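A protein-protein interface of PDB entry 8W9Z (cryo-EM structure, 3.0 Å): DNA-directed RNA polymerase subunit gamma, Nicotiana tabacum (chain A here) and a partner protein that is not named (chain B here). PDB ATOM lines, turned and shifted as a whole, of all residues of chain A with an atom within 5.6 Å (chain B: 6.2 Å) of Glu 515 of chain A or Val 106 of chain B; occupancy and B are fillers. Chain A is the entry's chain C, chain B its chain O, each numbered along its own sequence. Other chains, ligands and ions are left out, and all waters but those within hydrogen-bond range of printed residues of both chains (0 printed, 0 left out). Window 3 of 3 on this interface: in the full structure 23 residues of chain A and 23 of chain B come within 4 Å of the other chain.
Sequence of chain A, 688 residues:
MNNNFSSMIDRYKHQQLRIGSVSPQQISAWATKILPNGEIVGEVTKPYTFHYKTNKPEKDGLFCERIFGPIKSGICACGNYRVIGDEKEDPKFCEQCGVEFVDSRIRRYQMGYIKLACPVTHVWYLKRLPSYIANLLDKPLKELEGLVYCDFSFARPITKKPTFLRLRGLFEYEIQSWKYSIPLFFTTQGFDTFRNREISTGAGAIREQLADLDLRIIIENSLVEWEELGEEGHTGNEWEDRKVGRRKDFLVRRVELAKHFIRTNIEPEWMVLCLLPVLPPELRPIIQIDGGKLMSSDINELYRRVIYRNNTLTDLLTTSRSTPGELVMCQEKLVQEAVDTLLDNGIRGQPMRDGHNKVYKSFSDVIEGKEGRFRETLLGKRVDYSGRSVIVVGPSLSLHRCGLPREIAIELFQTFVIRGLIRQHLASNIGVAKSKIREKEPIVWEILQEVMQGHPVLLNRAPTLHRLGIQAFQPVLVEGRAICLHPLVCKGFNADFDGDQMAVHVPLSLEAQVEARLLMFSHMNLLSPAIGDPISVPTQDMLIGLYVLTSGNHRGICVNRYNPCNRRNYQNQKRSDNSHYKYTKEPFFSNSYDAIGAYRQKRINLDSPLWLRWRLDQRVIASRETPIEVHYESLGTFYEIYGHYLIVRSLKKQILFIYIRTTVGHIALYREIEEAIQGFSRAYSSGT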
ATOM      1  N   LEU A 510      -1.699  -6.056 -13.844  1.00  0.00           N
ATOM      2  CA  LEU A 510      -1.971  -7.487 -13.950  1.00  0.00           C
ATOM      3  C   LEU A 510      -0.743  -8.312 -13.591  1.00  0.00           C
ATOM      4  O   LEU A 510      -0.862  -9.363 -12.950  1.00  0.00           O
ATOM      5  CB  LEU A 510      -2.448  -7.831 -15.361  1.00  0.00           C
ATOM      6  CG  LEU A 510      -3.784  -7.237 -15.807  1.00  0.00           C
ATOM      7  CD1 LEU A 510      -4.125  -7.693 -17.216  1.00  0.00           C
ATOM      8  CD2 LEU A 510      -4.891  -7.613 -14.835  1.00  0.00           C
ATOM      9  N   GLU A 511       0.442  -7.856 -14.001  1.00  0.00           N
ATOM     10  CA  GLU A 511       1.664  -8.596 -13.701  1.00  0.00           C
ATOM     11  C   GLU A 511       1.896  -8.686 -12.199  1.00  0.00           C
ATOM     12  O   GLU A 511       2.272  -9.747 -11.685  1.00  0.00           O
ATOM     13  CB  GLU A 511       2.861  -7.942 -14.392  1.00  0.00           C
ATOM     14  CG  GLU A 511       2.799  -7.950 -15.914  1.00  0.00           C
ATOM     15  CD  GLU A 511       1.895  -6.869 -16.475  1.00  0.00           C
ATOM     16  OE1 GLU A 511       1.492  -5.971 -15.707  1.00  0.00           O
ATOM     17  OE2 GLU A 511       1.586  -6.918 -17.685  1.00  0.00           O
ATOM     18  N   ALA A 512       1.671  -7.584 -11.481  1.00  0.00           N
ATOM     19  CA  ALA A 512       1.832  -7.602 -10.031  1.00  0.00           C
ATOM     20  C   ALA A 512       0.849  -8.565  -9.380  1.00  0.00           C
ATOM     21  O   ALA A 512       1.209  -9.296  -8.450  1.00  0.00           O
ATOM     22  CB  ALA A 512       1.660  -6.193  -9.468  1.00  0.00           C
ATOM     23  N   GLN A 513      -0.396  -8.588  -9.862  1.00  0.00           N
ATOM     24  CA  GLN A 513      -1.388  -9.500  -9.303  1.00  0.00           C
ATOM     25  C   GLN A 513      -1.008 -10.954  -9.554  1.00  0.00           C
ATOM     26  O   GLN A 513      -1.129 -11.796  -8.656  1.00  0.00           O
ATOM     27  CB  GLN A 513      -2.767  -9.198  -9.883  1.00  0.00           C
ATOM     28  CG  GLN A 513      -3.300  -7.822  -9.529  1.00  0.00           C
ATOM     29  CD  GLN A 513      -4.649  -7.543 -10.156  1.00  0.00           C
ATOM     30  OE1 GLN A 513      -5.120  -6.407 -10.164  1.00  0.00           O
ATOM     31  NE2 GLN A 513      -5.281  -8.582 -10.686  1.00  0.00           N
ATOM     32  N   VAL A 514      -0.543 -11.269 -10.766  1.00  0.00           N
ATOM     33  CA  VAL A 514      -0.146 -12.642 -11.069  1.00  0.00           C
ATOM     34  C   VAL A 514       1.048 -13.054 -10.219  1.00  0.00           C
ATOM     35  O   VAL A 514       1.100 -14.173  -9.694  1.00  0.00           O
ATOM     36  CB  VAL A 514       0.148 -12.800 -12.572  1.00  0.00           C
ATOM     37  CG1 VAL A 514       0.632 -14.206 -12.869  1.00  0.00           C
ATOM     38  CG2 VAL A 514      -1.090 -12.493 -13.389  1.00  0.00           C
ATOM     39  N   GLU A 515       2.019 -12.152 -10.053  1.00  0.00           N
ATOM     40  CA  GLU A 515       3.185 -12.470  -9.234  1.00  0.00           C
ATOM     41  C   GLU A 515       2.801 -12.667  -7.774  1.00  0.00           C
ATOM     42  O   GLU A 515       3.343 -13.550  -7.098  1.00  0.00           O
ATOM     43  CB  GLU A 515       4.236 -11.370  -9.365  1.00  0.00           C
ATOM     44  CG  GLU A 515       4.902 -11.298 -10.723  1.00  0.00           C
ATOM     45  CD  GLU A 515       5.889 -10.155 -10.821  1.00  0.00           C
ATOM     46  OE1 GLU A 515       6.109  -9.470  -9.801  1.00  0.00           O
ATOM     47  OE2 GLU A 515       6.442  -9.938 -11.918  1.00  0.00           O
ATOM     48  N   ALA A 516       1.870 -11.856  -7.267  1.00  0.00           N
ATOM     49  CA  ALA A 516       1.456 -11.994  -5.876  1.00  0.00           C
ATOM     50  C   ALA A 516       0.631 -13.254  -5.655  1.00  0.00           C
ATOM     51  O   ALA A 516       0.699 -13.856  -4.578  1.00  0.00           O
ATOM     52  CB  ALA A 516       0.670 -10.761  -5.436  1.00  0.00           C
ATOM     53  N   ARG A 517      -0.150 -13.669  -6.653  1.00  0.00           N
ATOM     54  CA  ARG A 517      -0.989 -14.849  -6.487  1.00  0.00           C
ATOM     55  C   ARG A 517      -0.218 -16.143  -6.716  1.00  0.00           C
ATOM     56  O   ARG A 517      -0.574 -17.177  -6.142  1.00  0.00           O
ATOM     57  CB  ARG A 517      -2.189 -14.775  -7.434  1.00  0.00           C
ATOM     58  CG  ARG A 517      -3.239 -15.848  -7.192  1.00  0.00           C
ATOM     59  CD  ARG A 517      -4.392 -15.749  -8.181  1.00  0.00           C
ATOM     60  NE  ARG A 517      -5.222 -14.568  -7.958  1.00  0.00           N
ATOM     61  CZ  ARG A 517      -5.121 -13.439  -8.652  1.00  0.00           C
ATOM     62  NH1 ARG A 517      -4.224 -13.333  -9.623  1.00  0.00           N
ATOM     63  NH2 ARG A 517      -5.921 -12.418  -8.380  1.00  0.00           N
ATOM     64  N   LEU A 518       0.835 -16.113  -7.533  1.00  0.00           N
ATOM     65  CA  LEU A 518       1.548 -17.335  -7.881  1.00  0.00           C
ATOM     66  C   LEU A 518       2.870 -17.513  -7.147  1.00  0.00           C
ATOM     67  O   LEU A 518       3.374 -18.640  -7.088  1.00  0.00           O
ATOM     68  CB  LEU A 518       1.810 -17.389  -9.391  1.00  0.00           C
ATOM     69  CG  LEU A 518       0.698 -17.939 -10.290  1.00  0.00           C
ATOM     70  CD1 LEU A 518      -0.502 -17.009 -10.339  1.00  0.00           C
ATOM     71  CD2 LEU A 518       1.233 -18.199 -11.687  1.00  0.00           C
ATOM     72  N   LEU A 519       3.446 -16.452  -6.592  1.00  0.00           N
ATOM     73  CA  LEU A 519       4.757 -16.552  -5.959  1.00  0.00           C
ATOM     74  C   LEU A 519       4.767 -16.159  -4.491  1.00  0.00           C
ATOM     75  O   LEU A 519       5.417 -16.831  -3.687  1.00  0.00           O
ATOM     76  CB  LEU A 519       5.778 -15.688  -6.715  1.00  0.00           C
ATOM     77  CG  LEU A 519       6.134 -16.107  -8.142  1.00  0.00           C
ATOM     78  CD1 LEU A 519       7.175 -15.170  -8.725  1.00  0.00           C
ATOM     79  CD2 LEU A 519       6.626 -17.543  -8.172  1.00  0.00           C
ATOM     80  N   MET A 520       4.071 -15.091  -4.113  1.00  0.00           N
ATOM     81  CA  MET A 520       4.207 -14.517  -2.782  1.00  0.00           C
ATOM     82  C   MET A 520       3.217 -15.074  -1.768  1.00  0.00           C
ATOM     83  O   MET A 520       3.170 -14.576  -0.638  1.00  0.00           O
ATOM     84  CB  MET A 520       4.061 -12.994  -2.852  1.00  0.00           C
ATOM     85  CG  MET A 520       5.148 -12.308  -3.656  1.00  0.00           C
ATOM     86  SD  MET A 520       5.060 -10.514  -3.539  1.00  0.00           S
ATOM     87  CE  MET A 520       5.238 -10.294  -1.772  1.00  0.00           C
ATOM     88  N   ASN B 101      10.855 -23.320 -15.073  1.00  0.00           N
ATOM     89  CA  ASN B 101      10.963 -22.056 -14.361  1.00  0.00           C
ATOM     90  C   ASN B 101       9.584 -21.577 -13.931  1.00  0.00           C
ATOM     91  O   ASN B 101       8.623 -21.635 -14.704  1.00  0.00           O
ATOM     92  CB  ASN B 101      11.630 -20.994 -15.235  1.00  0.00           C
ATOM     93  CG  ASN B 101      13.067 -21.333 -15.572  1.00  0.00           C
ATOM     94  OD1 ASN B 101      13.418 -21.514 -16.738  1.00  0.00           O
ATOM     95  ND2 ASN B 101      13.911 -21.418 -14.551  1.00  0.00           N
ATOM     96  N   ARG B 102       9.493 -21.099 -12.694  1.00  0.00           N
ATOM     97  CA  ARG B 102       8.251 -20.551 -12.169  1.00  0.00           C
ATOM     98  C   ARG B 102       8.063 -19.085 -12.528  1.00  0.00           C
ATOM     99  O   ARG B 102       7.064 -18.484 -12.120  1.00  0.00           O
ATOM    100  CB  ARG B 102       8.194 -20.726 -10.649  1.00  0.00           C
ATOM    101  CG  ARG B 102       9.301 -20.012  -9.897  1.00  0.00           C
ATOM    102  CD  ARG B 102       9.209 -20.287  -8.406  1.00  0.00           C
ATOM    103  NE  ARG B 102      10.213 -19.544  -7.651  1.00  0.00           N
ATOM    104  CZ  ARG B 102      11.436 -19.993  -7.392  1.00  0.00           C
ATOM    105  NH1 ARG B 102      11.812 -21.186  -7.829  1.00  0.00           N
ATOM    106  NH2 ARG B 102      12.284 -19.249  -6.696  1.00  0.00           N
ATOM    107  N   PHE B 103       8.996 -18.499 -13.275  1.00  0.00           N
ATOM    108  CA  PHE B 103       8.895 -17.123 -13.745  1.00  0.00           C
ATOM    109  C   PHE B 103       8.347 -17.031 -15.161  1.00  0.00           C
ATOM    110  O   PHE B 103       7.536 -16.144 -15.455  1.00  0.00           O
ATOM    111  CB  PHE B 103      10.268 -16.449 -13.682  1.00  0.00           C
ATOM    112  CG  PHE B 103      10.938 -16.564 -12.343  1.00  0.00           C
ATOM    113  CD1 PHE B 103      10.211 -16.424 -11.174  1.00  0.00           C
ATOM    114  CD2 PHE B 103      12.294 -16.822 -12.254  1.00  0.00           C
ATOM    115  CE1 PHE B 103      10.827 -16.533  -9.943  1.00  0.00           C
ATOM    116  CE2 PHE B 103      12.913 -16.930 -11.025  1.00  0.00           C
ATOM    117  CZ  PHE B 103      12.179 -16.786  -9.870  1.00  0.00           C
ATOM    118  N   ASP B 104       8.773 -17.933 -16.047  1.00  0.00           N
ATOM    119  CA  ASP B 104       8.194 -17.985 -17.384  1.00  0.00           C
ATOM    120  C   ASP B 104       6.714 -18.333 -17.332  1.00  0.00           C
ATOM    121  O   ASP B 104       5.934 -17.846 -18.157  1.00  0.00           O
ATOM    122  CB  ASP B 104       8.951 -18.993 -18.247  1.00  0.00           C
ATOM    123  CG  ASP B 104      10.409 -18.627 -18.428  1.00  0.00           C
ATOM    124  OD1 ASP B 104      10.724 -17.418 -18.418  1.00  0.00           O
ATOM    125  OD2 ASP B 104      11.241 -19.546 -18.580  1.00  0.00           O
ATOM    126  N   PHE B 105       6.307 -19.159 -16.366  1.00  0.00           N
ATOM    127  CA  PHE B 105       4.890 -19.470 -16.207  1.00  0.00           C
ATOM    128  C   PHE B 105       4.096 -18.231 -15.812  1.00  0.00           C
ATOM    129  O   PHE B 105       3.006 -17.985 -16.345  1.00  0.00           O
ATOM    130  CB  PHE B 105       4.722 -20.580 -15.170  1.00  0.00           C
ATOM    131  CG  PHE B 105       3.325 -21.114 -15.070  1.00  0.00           C
ATOM    132  CD1 PHE B 105       2.731 -21.742 -16.150  1.00  0.00           C
ATOM    133  CD2 PHE B 105       2.613 -21.004 -13.889  1.00  0.00           C
ATOM    134  CE1 PHE B 105       1.446 -22.238 -16.059  1.00  0.00           C
ATOM    135  CE2 PHE B 105       1.330 -21.501 -13.790  1.00  0.00           C
ATOM    136  CZ  PHE B 105       0.745 -22.119 -14.877  1.00  0.00           C
ATOM    137  N   VAL B 106       4.635 -17.435 -14.885  1.00  0.00           N
ATOM    138  CA  VAL B 106       3.981 -16.190 -14.491  1.00  0.00           C
ATOM    139  C   VAL B 106       3.890 -15.239 -15.676  1.00  0.00           C
ATOM    140  O   VAL B 106       2.852 -14.605 -15.906  1.00  0.00           O
ATOM    141  CB  VAL B 106       4.729 -15.552 -13.306  1.00  0.00           C
ATOM    142  CG1 VAL B 106       4.259 -14.128 -13.078  1.00  0.00           C
ATOM    143  CG2 VAL B 106       4.537 -16.386 -12.051  1.00  0.00           C
ATOM    144  N   ASN B 107       4.972 -15.128 -16.450  1.00  0.00           N
ATOM    145  CA  ASN B 107       4.959 -14.247 -17.615  1.00  0.00           C
ATOM    146  C   ASN B 107       3.934 -14.707 -18.647  1.00  0.00           C
ATOM    147  O   ASN B 107       3.224 -13.884 -19.238  1.00  0.00           O
ATOM    148  CB  ASN B 107       6.353 -14.173 -18.234  1.00  0.00           C
ATOM    149  CG  ASN B 107       7.357 -13.495 -17.325  1.00  0.00           C
ATOM    150  OD1 ASN B 107       6.996 -12.647 -16.511  1.00  0.00           O
ATOM    151  ND2 ASN B 107       8.623 -13.865 -17.461  1.00  0.00           N
ATOM    152  N   GLU B 108       3.835 -16.020 -18.868  1.00  0.00           N
ATOM    153  CA  GLU B 108       2.872 -16.540 -19.833  1.00  0.00           C
ATOM    154  C   GLU B 108       1.442 -16.295 -19.373  1.00  0.00           C
ATOM    155  O   GLU B 108       0.580 -15.922 -20.179  1.00  0.00           O
ATOM    156  CB  GLU B 108       3.122 -18.030 -20.066  1.00  0.00           C
ATOM    157  CG  GLU B 108       2.348 -18.630 -21.233  1.00  0.00           C
ATOM    158  CD  GLU B 108       0.959 -19.103 -20.845  1.00  0.00           C
ATOM    159  OE1 GLU B 108       0.702 -19.271 -19.634  1.00  0.00           O
ATOM    160  OE2 GLU B 108       0.126 -19.307 -21.752  1.00  0.00           O
ATOM    161  N   ILE B 109       1.168 -16.494 -18.081  1.00  0.00           N
ATOM    162  CA  ILE B 109      -0.174 -16.237 -17.570  1.00  0.00           C
ATOM    163  C   ILE B 109      -0.514 -14.755 -17.679  1.00  0.00           C
ATOM    164  O   ILE B 109      -1.639 -14.391 -18.044  1.00  0.00           O
ATOM    165  CB  ILE B 109      -0.308 -16.747 -16.123  1.00  0.00           C
ATOM    166  CG1 ILE B 109      -0.333 -18.274 -16.104  1.00  0.00           C
ATOM    167  CG2 ILE B 109      -1.561 -16.190 -15.468  1.00  0.00           C
ATOM    168  CD1 ILE B 109      -0.699 -18.852 -14.764  1.00  0.00           C
ATOM    169  N   ALA B 110       0.448 -13.878 -17.381  1.00  0.00           N
ATOM    170  CA  ALA B 110       0.195 -12.446 -17.495  1.00  0.00           C
ATOM    171  C   ALA B 110      -0.074 -12.046 -18.940  1.00  0.00           C
ATOM    172  O   ALA B 110      -0.975 -11.245 -19.214  1.00  0.00           O
ATOM    173  CB  ALA B 110       1.374 -11.656 -16.927  1.00  0.00           C
ATOM    174  N   ALA B 111       0.690 -12.604 -19.883  1.00  0.00           N
ATOM    175  CA  ALA B 111       0.469 -12.297 -21.292  1.00  0.00           C
ATOM    176  C   ALA B 111      -0.893 -12.794 -21.761  1.00  0.00           C
ATOM    177  O   ALA B 111      -1.599 -12.087 -22.491  1.00  0.00           O
ATOM    178  CB  ALA B 111       1.583 -12.902 -22.143  1.00  0.00           C
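Glu 515 of chain A touches just one residue of chain B: Val 106.
Of the printed residues of chain A, Ile 109 of chain B touches Val 514 (3.9 Å) and Leu 518 (3.7 Å).
Printed residues of chain A within 4 Å of Arg 102 of chain B: Leu 519 (3.8 Å).
Printed residues of chain B within 4 Å of Leu 518 of chain A: Phe 105 (3.8 Å), Val 106 (3.8 Å) and Ile 109 (3.7 Å).
Printed residues of chain B within 4 Å of Leu 519 of chain A: Arg 102 (3.8 Å).
Of the printed residues of chain B, Val 514 of chain A touches Val 106 (3.6 Å) and Ile 109 (3.9 Å).
The nearest residue of chain B that does not touch Glu 515 of chain A is Asn 107 of chain B (5.4 Å).
The nearest residue of chain A that does not touch Val 106 of chain B is Leu 519 of chain A (4.2 Å).
Val 514 of chain A touches Val 106 of chain B (CG1 to CG1, 3.6 Å).
Val 514 of chain A touches Ile 109 of chain B.
Val 106 of chain B touches Glu 515 of chain A (CG1 to CG, 3.7 Å).
Phe 105 of chain B touches Leu 518 of chain A.
Leu 518 of chain A touches Val 106 of chain B (CD2 to CG2, 3.8 Å).
Leu 518 of chain A touches Ile 109 of chain B.
CD of Arg 102 of chain B touches CD2 of Leu 519 of chain A, at 3.8 Å.
Of the 11 printed residues of chain B, 4 touch a printed residue of chain A.
Printed residues of chain B that touch a printed residue of chain A: Arg 102, Phe 105, Val 106 and Ile 109.
Along chain B the printed residues that touch a printed residue of chain A span positions 102 to 109.
Of the 11 printed residues of chain A, 4 touch a printed residue of chain B.
Hydrophobic or aromatic side chains of chain A within 4 Å of the printed part of chain B: Val 514, Leu 518 and Leu 519.
The backbone NH (N) of Met 520 of chain A lies within hydrogen-bond range of the backbone carbonyl oxygen (O) of Glu 515 of chain A.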
